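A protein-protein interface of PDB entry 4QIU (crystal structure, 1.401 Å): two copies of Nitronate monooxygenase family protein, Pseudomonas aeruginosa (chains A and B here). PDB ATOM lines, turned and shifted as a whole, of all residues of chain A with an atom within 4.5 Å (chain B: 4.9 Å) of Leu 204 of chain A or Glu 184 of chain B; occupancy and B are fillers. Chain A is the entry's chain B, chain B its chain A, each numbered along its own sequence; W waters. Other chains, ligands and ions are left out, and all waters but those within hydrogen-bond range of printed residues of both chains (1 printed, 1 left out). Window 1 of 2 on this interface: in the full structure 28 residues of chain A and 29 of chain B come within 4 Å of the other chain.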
ATOM      1  N   GLY A 202      25.771  14.858  -3.297  1.00  0.00           N
ATOM      2  CA  GLY A 202      26.699  14.785  -4.413  1.00  0.00           C
ATOM      3  C   GLY A 202      27.376  16.114  -4.693  1.00  0.00           C
ATOM      4  O   GLY A 202      26.835  17.179  -4.375  1.00  0.00           O
ATOM      5  N   THR A 203      28.564  16.047  -5.291  1.00  0.00           N
ATOM      6  CA  THR A 203      29.345  17.233  -5.609  1.00  0.00           C
ATOM      7  C   THR A 203      28.557  18.280  -6.405  1.00  0.00           C
ATOM      8  O   THR A 203      28.595  19.474  -6.084  1.00  0.00           O
ATOM      9  CB  THR A 203      30.616  16.832  -6.384  1.00  0.00           C
ATOM     10  OG1 THR A 203      31.405  15.982  -5.545  1.00  0.00           O
ATOM     11  CG2 THR A 203      31.444  18.056  -6.767  1.00  0.00           C
ATOM     12  N   LEU A 204      27.832  17.852  -7.436  1.00  0.00           N
ATOM     13  CA  LEU A 204      27.146  18.813  -8.297  1.00  0.00           C
ATOM     14  C   LEU A 204      26.103  19.616  -7.518  1.00  0.00           C
ATOM     15  O   LEU A 204      25.995  20.830  -7.698  1.00  0.00           O
ATOM     16  CB  LEU A 204      26.507  18.105  -9.501  1.00  0.00           C
ATOM     17  CG  LEU A 204      25.786  19.005 -10.508  1.00  0.00           C
ATOM     18  CD1 LEU A 204      26.150  18.638 -11.936  1.00  0.00           C
ATOM     19  CD2 LEU A 204      24.275  18.936 -10.300  1.00  0.00           C
ATOM     20  N   ALA A 205      25.344  18.954  -6.652  1.00  0.00           N
ATOM     21  CA  ALA A 205      24.397  19.687  -5.806  1.00  0.00           C
ATOM     22  C   ALA A 205      25.117  20.516  -4.753  1.00  0.00           C
ATOM     23  O   ALA A 205      24.785  21.680  -4.559  1.00  0.00           O
ATOM     24  CB  ALA A 205      23.413  18.737  -5.130  1.00  0.00           C
ATOM     25  N   LEU A 206      26.092  19.929  -4.064  1.00  0.00           N
ATOM     26  CA  LEU A 206      26.706  20.633  -2.929  1.00  0.00           C
ATOM     27  C   LEU A 206      27.424  21.901  -3.349  1.00  0.00           C
ATOM     28  O   LEU A 206      27.272  22.936  -2.702  1.00  0.00           O
ATOM     29  CB  LEU A 206      27.681  19.721  -2.175  1.00  0.00           C
ATOM     30  CG  LEU A 206      28.333  20.330  -0.924  1.00  0.00           C
ATOM     31  CD1 LEU A 206      27.278  20.705   0.124  1.00  0.00           C
ATOM     32  CD2 LEU A 206      29.380  19.393  -0.328  1.00  0.00           C
ATOM     33  N   VAL A 207      28.205  21.826  -4.417  1.00  0.00           N
ATOM     34  CA  VAL A 207      28.964  22.988  -4.865  1.00  0.00           C
ATOM     35  C   VAL A 207      27.994  24.101  -5.259  1.00  0.00           C
ATOM     36  O   VAL A 207      28.184  25.264  -4.887  1.00  0.00           O
ATOM     37  CB  VAL A 207      29.892  22.633  -6.050  1.00  0.00           C
ATOM     38  CG1 VAL A 207      30.532  23.890  -6.601  1.00  0.00           C
ATOM     39  CG2 VAL A 207      30.970  21.662  -5.593  1.00  0.00           C
ATOM     40  N   ARG A 208      26.942  23.744  -5.987  1.00  0.00           N
ATOM     41  CA  ARG A 208      25.960  24.744  -6.407  1.00  0.00           C
ATOM     42  C   ARG A 208      25.261  25.363  -5.200  1.00  0.00           C
ATOM     43  O   ARG A 208      25.062  26.575  -5.147  1.00  0.00           O
ATOM     44  CB  ARG A 208      24.934  24.138  -7.354  1.00  0.00           C
ATOM     45  CG  ARG A 208      24.053  25.172  -8.044  1.00  0.00           C
ATOM     46  CD  ARG A 208      24.778  25.928  -9.170  1.00  0.00           C
ATOM     47  NE  ARG A 208      24.114  27.215  -9.410  1.00  0.00           N
ATOM     48  CZ  ARG A 208      24.571  28.397  -9.003  1.00  0.00           C
ATOM     49  NH1 ARG A 208      25.743  28.502  -8.387  1.00  0.00           N
ATOM     50  NH2 ARG A 208      23.867  29.496  -9.257  1.00  0.00           N
ATOM     51  N   LEU A 236      29.567  25.641 -11.840  1.00  0.00           N
ATOM     52  CA  LEU A 236      28.685  25.560 -10.675  1.00  0.00           C
ATOM     53  C   LEU A 236      28.919  26.689  -9.682  1.00  0.00           C
ATOM     54  O   LEU A 236      28.135  26.870  -8.745  1.00  0.00           O
ATOM     55  CB  LEU A 236      28.874  24.221  -9.969  1.00  0.00           C
ATOM     56  CG  LEU A 236      28.454  22.998 -10.786  1.00  0.00           C
ATOM     57  CD1 LEU A 236      28.896  21.731 -10.062  1.00  0.00           C
ATOM     58  CD2 LEU A 236      26.947  22.973 -11.043  1.00  0.00           C
ATOM     59  N   GLY B 182      22.096  10.547 -11.330  1.00  0.00           N
ATOM     60  CA  GLY B 182      23.008  10.638 -10.206  1.00  0.00           C
ATOM     61  C   GLY B 182      22.278  10.490  -8.884  1.00  0.00           C
ATOM     62  O   GLY B 182      21.039  10.545  -8.838  1.00  0.00           O
ATOM     63  N   ILE B 183      23.049  10.304  -7.810  1.00  0.00           N
ATOM     64  CA  ILE B 183      22.485  10.117  -6.476  1.00  0.00           C
ATOM     65  C   ILE B 183      21.663  11.341  -6.047  1.00  0.00           C
ATOM     66  O   ILE B 183      20.740  11.210  -5.241  1.00  0.00           O
ATOM     67  CB  ILE B 183      23.608   9.808  -5.429  1.00  0.00           C
ATOM     68  CG1 ILE B 183      23.033   9.190  -4.140  1.00  0.00           C
ATOM     69  CG2 ILE B 183      24.429  11.038  -5.133  1.00  0.00           C
ATOM     70  CD1 ILE B 183      22.172   7.950  -4.334  1.00  0.00           C
ATOM     71  N   GLU B 184      21.969  12.502  -6.627  1.00  0.00           N
ATOM     72  CA  GLU B 184      21.231  13.744  -6.350  1.00  0.00           C
ATOM     73  C   GLU B 184      19.756  13.659  -6.706  1.00  0.00           C
ATOM     74  O   GLU B 184      18.948  14.413  -6.163  1.00  0.00           O
ATOM     75  CB  GLU B 184      21.828  14.926  -7.128  1.00  0.00           C
ATOM     76  CG  GLU B 184      23.128  15.493  -6.578  1.00  0.00           C
ATOM     77  CD  GLU B 184      24.374  14.857  -7.150  1.00  0.00           C
ATOM     78  OE1 GLU B 184      24.350  13.653  -7.492  1.00  0.00           O
ATOM     79  OE2 GLU B 184      25.386  15.582  -7.243  1.00  0.00           O
ATOM     80  N   ALA B 185      19.406  12.793  -7.653  1.00  0.00           N
ATOM     81  CA  ALA B 185      18.074  12.838  -8.248  1.00  0.00           C
ATOM     82  C   ALA B 185      16.939  12.592  -7.277  1.00  0.00           C
ATOM     83  O   ALA B 185      17.055  11.789  -6.360  1.00  0.00           O
ATOM     84  CB  ALA B 185      17.985  11.851  -9.375  1.00  0.00           C
ATOM     85  N   GLY B 186      15.832  13.300  -7.498  1.00  0.00           N
ATOM     86  CA  GLY B 186      14.612  13.051  -6.761  1.00  0.00           C
ATOM     87  C   GLY B 186      13.855  11.845  -7.295  1.00  0.00           C
ATOM     88  O   GLY B 186      14.056  11.404  -8.429  1.00  0.00           O
ATOM     89  N   GLY B 202      27.351   9.859  -7.643  1.00  0.00           N
ATOM     90  CA  GLY B 202      26.949  11.245  -7.839  1.00  0.00           C
ATOM     91  C   GLY B 202      26.902  11.637  -9.311  1.00  0.00           C
ATOM     92  O   GLY B 202      27.626  11.083 -10.142  1.00  0.00           O
ATOM     93  N   THR B 203      26.055  12.607  -9.631  1.00  0.00           N
ATOM     94  CA  THR B 203      25.918  13.082 -11.008  1.00  0.00           C
ATOM     95  C   THR B 203      27.246  13.484 -11.655  1.00  0.00           C
ATOM     96  O   THR B 203      27.504  13.132 -12.810  1.00  0.00           O
ATOM     97  CB  THR B 203      24.958  14.285 -11.055  1.00  0.00           C
ATOM     98  OG1 THR B 203      23.688  13.890 -10.533  1.00  0.00           O
ATOM     99  CG2 THR B 203      24.786  14.795 -12.478  1.00  0.00           C
ATOM    100  N   LEU B 204      28.092  14.207 -10.929  1.00  0.00           N
ATOM    101  CA  LEU B 204      29.319  14.726 -11.514  1.00  0.00           C
ATOM    102  C   LEU B 204      30.222  13.577 -11.953  1.00  0.00           C
ATOM    103  O   LEU B 204      30.823  13.630 -13.031  1.00  0.00           O
ATOM    104  CB  LEU B 204      30.034  15.654 -10.528  1.00  0.00           C
ATOM    105  CG  LEU B 204      31.350  16.238 -11.063  1.00  0.00           C
ATOM    106  CD1 LEU B 204      31.379  17.730 -10.816  1.00  0.00           C
ATOM    107  CD2 LEU B 204      32.557  15.545 -10.422  1.00  0.00           C
ATOM    108  N   GLY B 222      19.849  14.813 -12.211  1.00  0.00           N
ATOM    109  CA  GLY B 222      20.037  14.746 -10.767  1.00  0.00           C
ATOM    110  C   GLY B 222      20.746  15.962 -10.207  1.00  0.00           C
ATOM    111  O   GLY B 222      21.958  16.117 -10.351  1.00  0.00           O
ATOM    112  N   GLY B 223      19.977  16.836  -9.571  1.00  0.00           N
ATOM    113  CA  GLY B 223      20.543  17.979  -8.879  1.00  0.00           C
ATOM    114  C   GLY B 223      20.666  19.248  -9.706  1.00  0.00           C
ATOM    115  O   GLY B 223      21.111  20.282  -9.204  1.00  0.00           O
ATOM    116  N   ILE B 224      20.260  19.183 -10.968  1.00  0.00           N
ATOM    117  CA  ILE B 224      20.377  20.323 -11.870  1.00  0.00           C
ATOM    118  C   ILE B 224      19.146  21.225 -11.766  1.00  0.00           C
ATOM    119  O   ILE B 224      18.031  20.782 -12.014  1.00  0.00           O
ATOM    120  CB  ILE B 224      20.584  19.836 -13.306  1.00  0.00           C
ATOM    121  CG1 ILE B 224      21.893  19.026 -13.356  1.00  0.00           C
ATOM    122  CG2 ILE B 224      20.651  21.016 -14.269  1.00  0.00           C
ATOM    123  CD1 ILE B 224      22.091  18.181 -14.611  1.00  0.00           C
ATOM    124  N   GLY B 229      24.051  24.731 -13.641  1.00  0.00           N
ATOM    125  CA  GLY B 229      24.056  23.272 -13.560  1.00  0.00           C
ATOM    126  C   GLY B 229      24.012  22.608 -14.927  1.00  0.00           C
ATOM    127  O   GLY B 229      24.688  21.605 -15.158  1.00  0.00           O
ATOM    128  N   ALA B 232      27.463  23.024 -16.388  1.00  0.00           N
ATOM    129  CA  ALA B 232      28.373  22.075 -15.752  1.00  0.00           C
ATOM    130  C   ALA B 232      28.202  20.676 -16.336  1.00  0.00           C
ATOM    131  O   ALA B 232      29.190  19.990 -16.616  1.00  0.00           O
ATOM    132  CB  ALA B 232      28.157  22.052 -14.228  1.00  0.00           C
ATOM    133  N   LEU B 236      30.948  18.299 -18.523  1.00  0.00           N
ATOM    134  CA  LEU B 236      31.280  16.915 -18.194  1.00  0.00           C
ATOM    135  C   LEU B 236      31.115  15.978 -19.380  1.00  0.00           C
ATOM    136  O   LEU B 236      31.562  14.828 -19.346  1.00  0.00           O
ATOM    137  CB  LEU B 236      30.403  16.434 -17.039  1.00  0.00           C
ATOM    138  CG  LEU B 236      30.654  17.173 -15.733  1.00  0.00           C
ATOM    139  CD1 LEU B 236      29.581  16.765 -14.726  1.00  0.00           C
ATOM    140  CD2 LEU B 236      32.049  16.856 -15.184  1.00  0.00           C
ATOM    141  N   ARG B 283      14.150   9.177  -3.314  1.00  0.00           N
ATOM    142  CA  ARG B 283      14.560  10.388  -2.609  1.00  0.00           C
ATOM    143  C   ARG B 283      13.456  11.428  -2.498  1.00  0.00           C
ATOM    144  O   ARG B 283      12.860  11.826  -3.496  1.00  0.00           O
ATOM    145  CB  ARG B 283      15.765  11.035  -3.299  1.00  0.00           C
ATOM    146  CG  ARG B 283      16.222  12.314  -2.560  1.00  0.00           C
ATOM    147  CD  ARG B 283      17.434  13.036  -3.218  1.00  0.00           C
ATOM    148  NE  ARG B 283      18.587  12.136  -3.308  1.00  0.00           N
ATOM    149  CZ  ARG B 283      19.320  11.756  -2.267  1.00  0.00           C
ATOM    150  NH1 ARG B 283      19.049  12.213  -1.040  1.00  0.00           N
ATOM    151  NH2 ARG B 283      20.317  10.910  -2.451  1.00  0.00           N
ATOM    152  N   GLY B 332      14.936  16.295  -5.373  1.00  0.00           N
ATOM    153  CA  GLY B 332      16.357  16.024  -5.499  1.00  0.00           C
ATOM    154  C   GLY B 332      17.182  16.889  -4.560  1.00  0.00           C
ATOM    155  O   GLY B 332      16.650  17.754  -3.844  1.00  0.00           O
ATOM    156  N   GLN B 333      18.493  16.679  -4.574  1.00  0.00           N
ATOM    157  CA  GLN B 333      19.360  17.340  -3.604  1.00  0.00           C
ATOM    158  C   GLN B 333      19.580  18.818  -3.928  1.00  0.00           C
ATOM    159  O   GLN B 333      20.160  19.542  -3.121  1.00  0.00           O
ATOM    160  CB  GLN B 333      20.691  16.590  -3.494  1.00  0.00           C
ATOM    161  CG  GLN B 333      20.543  15.240  -2.775  1.00  0.00           C
ATOM    162  CD  GLN B 333      21.866  14.518  -2.616  1.00  0.00           C
ATOM    163  OE1 GLN B 333      22.781  14.696  -3.422  1.00  0.00           O
ATOM    164  NE2 GLN B 333      21.992  13.730  -1.551  1.00  0.00           N
HETATM  165  O   HOH W   1      23.357  21.968  -9.046  1.00  0.00           O
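Of the 17 printed residues of chain B, 7 touch a printed residue of chain A.
Printed residues of chain B that touch a printed residue of chain A: Glu 184, Gly 222, Gly 223, Ile 224, Gly 229, Ala 232 and Gln 333.
Hydrophobic or aromatic side chains of chain B within 4 Å of the printed part of chain A: Ile 224 and Ala 232.
Printed residues of chain A that touch a printed residue of chain B: Gly 202, Thr 203, Leu 204, Ala 205 and Leu 236.
Hydrophobic or aromatic side chains of chain A within 4 Å of the printed part of chain B: Leu 204, Ala 205 and Leu 236.
Among the printed residues, 11 pairs touch across the chains.
The side-chain amide oxygen (OE1) of Gln 333 of chain B is in hydrogen-bond range of the backbone NH (N) of Gly 202 of chain A (3.0 Å).
The side-chain carboxylate of Glu 184 of chain B sits at hydrogen-bond distance from the backbone NH of Ala 205 of chain A, at 3.4 Å.
The side-chain carboxylate (OE2) of Glu 184 of chain B lies within hydrogen-bond range of the backbone NH (N) of Leu 204 of chain A (3.3 Å).
4 positions are printed for both chains.
Of the 11 pairs that touch across the chains among the printed residues, none has its exchanged pair printed and touching as well.
Leu 204 of chain A touches just these residues of chain B: Glu 184, Gly 222, Gly 223 and Ile 224.
Of the printed residues of chain B, Ala 205 of chain A touches Glu 184 and Gln 333.
Val 207 of chain A touches none of the printed residues of chain B.
Arg 208 of chain A touches none of the printed residues of chain B.
Glu 184 of chain B touches just these residues of chain A: Gly 202, Thr 203, Leu 204 and Ala 205.
Of the printed residues of chain A, Gly 222 of chain B touches Leu 204.
Of the printed residues of chain A, Ile 224 of chain B touches Leu 204.
Of the printed residues of chain A, Gly 229 of chain B touches Leu 236.
Of the printed residues of chain A, Gln 333 of chain B touches Gly 202 (3.0 Å) and Ala 205 (3.8 Å).
Among the printed residues, merely in contact across the chains: Gly 202 of chain A with Glu 184 of chain B (3.2 Å), Leu 236 of chain A with Ala 232 of chain B (3.5 Å), Leu 204 of chain A with Gly 223 of chain B (3.6 Å), Leu 204 of chain A with Gly 222 of chain B (3.6 Å), Thr 203 of chain A with Glu 184 of chain B (3.8 Å), Ala 205 of chain A with Gln 333 of chain B (3.8 Å), Leu 236 of chain A with Gly 229 of chain B (3.8 Å) and Leu 204 of chain A with Ile 224 of chain B (3.9 Å).
The backbone carbonyl oxygen of Glu 184 of chain B sits at hydrogen-bond distance from the backbone NH of Gln 333 of chain B (2.8 Å).
The guanidinium group (NH1) of Arg 208 of chain A sits at hydrogen-bond distance from the backbone carbonyl oxygen (O) of Leu 236 of chain A (2.9 Å).
The backbone carbonyl oxygen (O) of Gly 222 of chain B sits at hydrogen-bond distance from the side-chain hydroxyl (OG1) of Thr 203 of chain B (2.8 Å).
The side-chain amide nitrogen of Gln 333 of chain B sits close to the guanidinium group of Arg 283 of chain B (3.4 Å).
N of Thr 203 of chain B lies within hydrogen-bond range of OE1 of Glu 184 of chain B (2.9 Å).
Water W1 lies within hydrogen-bond range of O of Gly 223 of chain B and O of Leu 204 of chain A.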
